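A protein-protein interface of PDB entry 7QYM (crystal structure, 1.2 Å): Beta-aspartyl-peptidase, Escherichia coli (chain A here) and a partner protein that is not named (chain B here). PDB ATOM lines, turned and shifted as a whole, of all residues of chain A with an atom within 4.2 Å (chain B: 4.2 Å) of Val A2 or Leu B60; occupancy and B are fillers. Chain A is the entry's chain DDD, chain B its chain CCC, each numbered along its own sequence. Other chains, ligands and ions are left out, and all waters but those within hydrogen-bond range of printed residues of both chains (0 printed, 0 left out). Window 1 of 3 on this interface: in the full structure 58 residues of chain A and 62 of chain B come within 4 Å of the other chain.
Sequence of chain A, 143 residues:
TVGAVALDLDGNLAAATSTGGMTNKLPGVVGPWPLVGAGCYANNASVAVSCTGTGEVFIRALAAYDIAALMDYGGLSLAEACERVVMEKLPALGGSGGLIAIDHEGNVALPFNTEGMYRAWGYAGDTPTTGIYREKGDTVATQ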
ATOM      1  N   THR A   1      -5.577 -31.040 -20.573  1.00  0.00           N
ATOM      2  CA  THR A   1      -4.738 -30.227 -19.688  1.00  0.00           C
ATOM      3  C   THR A   1      -3.283 -30.482 -20.018  1.00  0.00           C
ATOM      4  O   THR A   1      -2.892 -31.614 -20.307  1.00  0.00           O
ATOM      5  CB  THR A   1      -5.039 -30.513 -18.214  1.00  0.00           C
ATOM      6  OG1 THR A   1      -6.466 -30.423 -18.128  1.00  0.00           O
ATOM      7  CG2 THR A   1      -4.332 -29.570 -17.267  1.00  0.00           C
ATOM      8  N   VAL A   2      -2.527 -29.413 -19.953  1.00  0.00           N
ATOM      9  CA  VAL A   2      -1.066 -29.417 -20.127  1.00  0.00           C
ATOM     10  C   VAL A   2      -0.489 -28.534 -19.045  1.00  0.00           C
ATOM     11  O   VAL A   2      -1.172 -27.699 -18.476  1.00  0.00           O
ATOM     12  CB  VAL A   2      -0.674 -28.902 -21.525  1.00  0.00           C
ATOM     13  CG1 VAL A   2      -1.373 -29.701 -22.615  1.00  0.00           C
ATOM     14  CG2 VAL A   2      -0.907 -27.412 -21.686  1.00  0.00           C
ATOM     15  N   GLY A   3       0.808 -28.670 -18.840  1.00  0.00           N
ATOM     16  CA  GLY A   3       1.463 -27.827 -17.858  1.00  0.00           C
ATOM     17  C   GLY A   3       2.969 -27.891 -17.917  1.00  0.00           C
ATOM     18  O   GLY A   3       3.528 -28.760 -18.594  1.00  0.00           O
ATOM     19  N   THR A  17      -0.295 -23.851 -16.313  1.00  0.00           N
ATOM     20  CA  THR A  17      -1.266 -24.899 -16.696  1.00  0.00           C
ATOM     21  C   THR A  17      -2.197 -24.314 -17.741  1.00  0.00           C
ATOM     22  O   THR A  17      -2.551 -23.140 -17.627  1.00  0.00           O
ATOM     23  CB  THR A  17      -2.131 -25.390 -15.524  1.00  0.00           C
ATOM     24  OG1 THR A  17      -2.921 -24.292 -15.043  1.00  0.00           O
ATOM     25  CG2 THR A  17      -1.293 -25.988 -14.426  1.00  0.00           C
ATOM     26  N   SER A  18      -2.625 -25.127 -18.694  1.00  0.00           N
ATOM     27  CA  SER A  18      -3.628 -24.679 -19.666  1.00  0.00           C
ATOM     28  C   SER A  18      -4.500 -25.872 -20.007  1.00  0.00           C
ATOM     29  O   SER A  18      -4.008 -26.984 -20.038  1.00  0.00           O
ATOM     30  CB  SER A  18      -2.946 -24.069 -20.871  1.00  0.00           C
ATOM     31  OG  SER A  18      -3.880 -23.529 -21.788  1.00  0.00           O
ATOM     32  N   HIS B   9       3.855 -31.689 -18.719  1.00  0.00           N
ATOM     33  CA  HIS B   9       2.879 -32.774 -18.864  1.00  0.00           C
ATOM     34  C   HIS B   9       1.868 -32.366 -19.922  1.00  0.00           C
ATOM     35  O   HIS B   9       1.663 -31.165 -20.196  1.00  0.00           O
ATOM     36  CB  HIS B   9       2.203 -33.137 -17.533  1.00  0.00           C
ATOM     37  CG  HIS B   9       1.164 -32.175 -17.098  1.00  0.00           C
ATOM     38  ND1 HIS B   9      -0.087 -32.183 -17.660  1.00  0.00           N
ATOM     39  CD2 HIS B   9       1.190 -31.179 -16.194  1.00  0.00           C
ATOM     40  CE1 HIS B   9      -0.777 -31.209 -17.117  1.00  0.00           C
ATOM     41  NE2 HIS B   9      -0.040 -30.594 -16.195  1.00  0.00           N
ATOM     42  N   GLY B  10       1.280 -33.393 -20.506  1.00  0.00           N
ATOM     43  CA  GLY B  10       0.196 -33.274 -21.465  1.00  0.00           C
ATOM     44  C   GLY B  10      -1.033 -33.989 -21.027  1.00  0.00           C
ATOM     45  O   GLY B  10      -1.820 -34.366 -21.903  1.00  0.00           O
ATOM     46  N   ILE B  35       9.469 -29.967 -26.926  1.00  0.00           N
ATOM     47  CA  ILE B  35       9.072 -28.876 -26.007  1.00  0.00           C
ATOM     48  C   ILE B  35      10.027 -28.850 -24.812  1.00  0.00           C
ATOM     49  O   ILE B  35      10.478 -27.762 -24.426  1.00  0.00           O
ATOM     50  CB  ILE B  35       7.594 -28.997 -25.634  1.00  0.00           C
ATOM     51  CG1 ILE B  35       6.761 -28.814 -26.906  1.00  0.00           C
ATOM     52  CG2 ILE B  35       7.236 -28.001 -24.556  1.00  0.00           C
ATOM     53  CD1 ILE B  35       5.333 -29.179 -26.768  1.00  0.00           C
ATOM     54  N   ALA B  56       6.723 -23.090 -22.823  1.00  0.00           N
ATOM     55  CA  ALA B  56       6.418 -24.533 -22.896  1.00  0.00           C
ATOM     56  C   ALA B  56       4.911 -24.732 -23.022  1.00  0.00           C
ATOM     57  O   ALA B  56       4.467 -25.554 -23.842  1.00  0.00           O
ATOM     58  CB  ALA B  56       6.980 -25.238 -21.706  1.00  0.00           C
ATOM     59  N   VAL B  57       4.155 -24.041 -22.174  1.00  0.00           N
ATOM     60  CA  VAL B  57       2.686 -24.227 -22.239  1.00  0.00           C
ATOM     61  C   VAL B  57       2.149 -23.638 -23.537  1.00  0.00           C
ATOM     62  O   VAL B  57       1.232 -24.221 -24.105  1.00  0.00           O
ATOM     63  CB  VAL B  57       2.026 -23.679 -20.970  1.00  0.00           C
ATOM     64  CG1 VAL B  57       0.526 -23.656 -21.137  1.00  0.00           C
ATOM     65  CG2 VAL B  57       2.391 -24.550 -19.784  1.00  0.00           C
ATOM     66  N   ARG B  58       2.715 -22.547 -24.028  1.00  0.00           N
ATOM     67  CA  ARG B  58       2.278 -22.041 -25.332  1.00  0.00           C
ATOM     68  C   ARG B  58       2.503 -23.114 -26.397  1.00  0.00           C
ATOM     69  O   ARG B  58       1.624 -23.313 -27.274  1.00  0.00           O
ATOM     70  CB  ARG B  58       3.000 -20.740 -25.684  1.00  0.00           C
ATOM     71  CG  ARG B  58       2.435 -20.074 -26.939  1.00  0.00           C
ATOM     72  CD  ARG B  58       3.329 -19.022 -27.541  1.00  0.00           C
ATOM     73  NE  ARG B  58       4.562 -19.578 -28.101  1.00  0.00           N
ATOM     74  CZ  ARG B  58       4.682 -20.153 -29.306  1.00  0.00           C
ATOM     75  NH1 ARG B  58       3.665 -20.197 -30.165  1.00  0.00           N
ATOM     76  NH2 ARG B  58       5.838 -20.677 -29.665  1.00  0.00           N
ATOM     77  N   LEU B  59       3.631 -23.810 -26.379  1.00  0.00           N
ATOM     78  CA  LEU B  59       3.893 -24.864 -27.372  1.00  0.00           C
ATOM     79  C   LEU B  59       2.931 -26.032 -27.202  1.00  0.00           C
ATOM     80  O   LEU B  59       2.533 -26.620 -28.200  1.00  0.00           O
ATOM     81  CB  LEU B  59       5.339 -25.313 -27.252  1.00  0.00           C
ATOM     82  CG  LEU B  59       6.376 -24.294 -27.732  1.00  0.00           C
ATOM     83  CD1 LEU B  59       7.759 -24.700 -27.310  1.00  0.00           C
ATOM     84  CD2 LEU B  59       6.292 -24.125 -29.233  1.00  0.00           C
ATOM     85  N   LEU B  60       2.595 -26.385 -25.977  1.00  0.00           N
ATOM     86  CA  LEU B  60       1.641 -27.489 -25.729  1.00  0.00           C
ATOM     87  C   LEU B  60       0.248 -27.069 -26.191  1.00  0.00           C
ATOM     88  O   LEU B  60      -0.509 -27.910 -26.717  1.00  0.00           O
ATOM     89  CB  LEU B  60       1.670 -27.847 -24.248  1.00  0.00           C
ATOM     90  CG  LEU B  60       2.961 -28.524 -23.796  1.00  0.00           C
ATOM     91  CD1 LEU B  60       3.155 -28.385 -22.286  1.00  0.00           C
ATOM     92  CD2 LEU B  60       2.955 -29.987 -24.205  1.00  0.00           C
ATOM     93  N   GLU B  61      -0.090 -25.790 -26.025  1.00  0.00           N
ATOM     94  CA  GLU B  61      -1.341 -25.253 -26.605  1.00  0.00           C
ATOM     95  C   GLU B  61      -1.304 -25.390 -28.130  1.00  0.00           C
ATOM     96  O   GLU B  61      -2.263 -25.858 -28.726  1.00  0.00           O
ATOM     97  CB  GLU B  61      -1.499 -23.784 -26.220  1.00  0.00           C
ATOM     98  CG  GLU B  61      -1.923 -23.590 -24.775  1.00  0.00           C
ATOM     99  CD  GLU B  61      -2.003 -22.128 -24.352  1.00  0.00           C
ATOM    100  OE1 GLU B  61      -1.533 -21.237 -25.122  1.00  0.00           O
ATOM    101  OE2 GLU B  61      -2.526 -21.826 -23.247  1.00  0.00           O
ATOM    102  N   GLU B  62      -0.229 -24.956 -28.756  1.00  0.00           N
ATOM    103  CA  GLU B  62      -0.167 -24.977 -30.233  1.00  0.00           C
ATOM    104  C   GLU B  62      -0.204 -26.404 -30.777  1.00  0.00           C
ATOM    105  O   GLU B  62      -0.728 -26.619 -31.858  1.00  0.00           O
ATOM    106  CB  GLU B  62       1.088 -24.282 -30.686  1.00  0.00           C
ATOM    107  CG  GLU B  62       1.039 -22.785 -30.460  1.00  0.00           C
ATOM    108  CD  GLU B  62      -0.059 -22.126 -31.280  1.00  0.00           C
ATOM    109  OE1 GLU B  62       0.016 -22.220 -32.537  1.00  0.00           O
ATOM    110  OE2 GLU B  62      -0.973 -21.525 -30.676  1.00  0.00           O
ATOM    111  N   CYS B  63       0.282 -27.364 -30.016  1.00  0.00           N
ATOM    112  CA  CYS B  63       0.344 -28.756 -30.447  1.00  0.00           C
ATOM    113  C   CYS B  63      -1.057 -29.343 -30.441  1.00  0.00           C
ATOM    114  O   CYS B  63      -1.644 -29.486 -29.368  1.00  0.00           O
ATOM    115  CB  CYS B  63       1.280 -29.510 -29.522  1.00  0.00           C
ATOM    116  SG  CYS B  63       1.436 -31.221 -30.040  1.00  0.00           S
ATOM    117  N   PHE B  66      -2.498 -32.201 -27.784  1.00  0.00           N
ATOM    118  CA  PHE B  66      -2.782 -31.951 -26.363  1.00  0.00           C
ATOM    119  C   PHE B  66      -3.983 -31.052 -26.190  1.00  0.00           C
ATOM    120  O   PHE B  66      -4.141 -30.067 -26.920  1.00  0.00           O
ATOM    121  CB  PHE B  66      -1.550 -31.410 -25.658  1.00  0.00           C
ATOM    122  CG  PHE B  66      -0.368 -32.335 -25.744  1.00  0.00           C
ATOM    123  CD1 PHE B  66      -0.375 -33.548 -25.085  1.00  0.00           C
ATOM    124  CD2 PHE B  66       0.751 -31.994 -26.472  1.00  0.00           C
ATOM    125  CE1 PHE B  66       0.671 -34.435 -25.213  1.00  0.00           C
ATOM    126  CE2 PHE B  66       1.827 -32.871 -26.548  1.00  0.00           C
ATOM    127  CZ  PHE B  66       1.785 -34.081 -25.922  1.00  0.00           C
ATOM    128  N   ALA B  68      -5.401 -28.435 -24.881  1.00  0.00           N
ATOM    129  CA  ALA B  68      -5.165 -27.049 -24.470  1.00  0.00           C
ATOM    130  C   ALA B  68      -5.006 -26.279 -25.775  1.00  0.00           C
ATOM    131  O   ALA B  68      -4.388 -26.821 -26.676  1.00  0.00           O
ATOM    132  CB  ALA B  68      -3.906 -26.904 -23.637  1.00  0.00           C
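Among the printed residues, merely in contact across the chains: Val A2 with His B9, Val A2 with Phe B66, Ser A18 with Val B57, Ser A18 with Ala B68, Val A2 with Ala B68, Val A2 with Leu B60, Gly A3 with Leu B60, Thr A1 with His B9 and Gly A3 with Val B57.
Along chain A the printed residues that touch a printed residue of chain B span positions 1 to 18. Printed residues of chain B that touch a printed residue of chain A: His B9, Gly B10, Val B57, Leu B60, Glu B61, Phe B66 and Ala B68.
N of Val A2 sits at hydrogen-bond distance from O of Ser A18 (2.8 Å).
Of the printed residues of chain A, Leu B60 touches Val A2 (3.7 Å) and Gly A3 (3.7 Å). Of the printed residues of chain A, His B9 touches Thr A1, Val A2 and Gly A3. Of the printed residues of chain B, Gly A3 touches His B9, Val B57 and Leu B60. The nearest printed residue of chain B that does not touch Val A2 is Val B57 (4.1 Å). The nearest printed residue of chain A that does not touch Val B57 is Val A2 (4.1 Å).
The side-chain carboxylate (OE2) of Glu B61 lies within hydrogen-bond range of the side-chain hydroxyl (OG) of Ser A18 (2.6 Å). The backbone NH (N) of His B9 lies within hydrogen-bond range of the backbone carbonyl oxygen (O) of Gly A3, 2.9 Å away. O of Thr A1 lies close to O of Gly B10 (3.4 Å).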
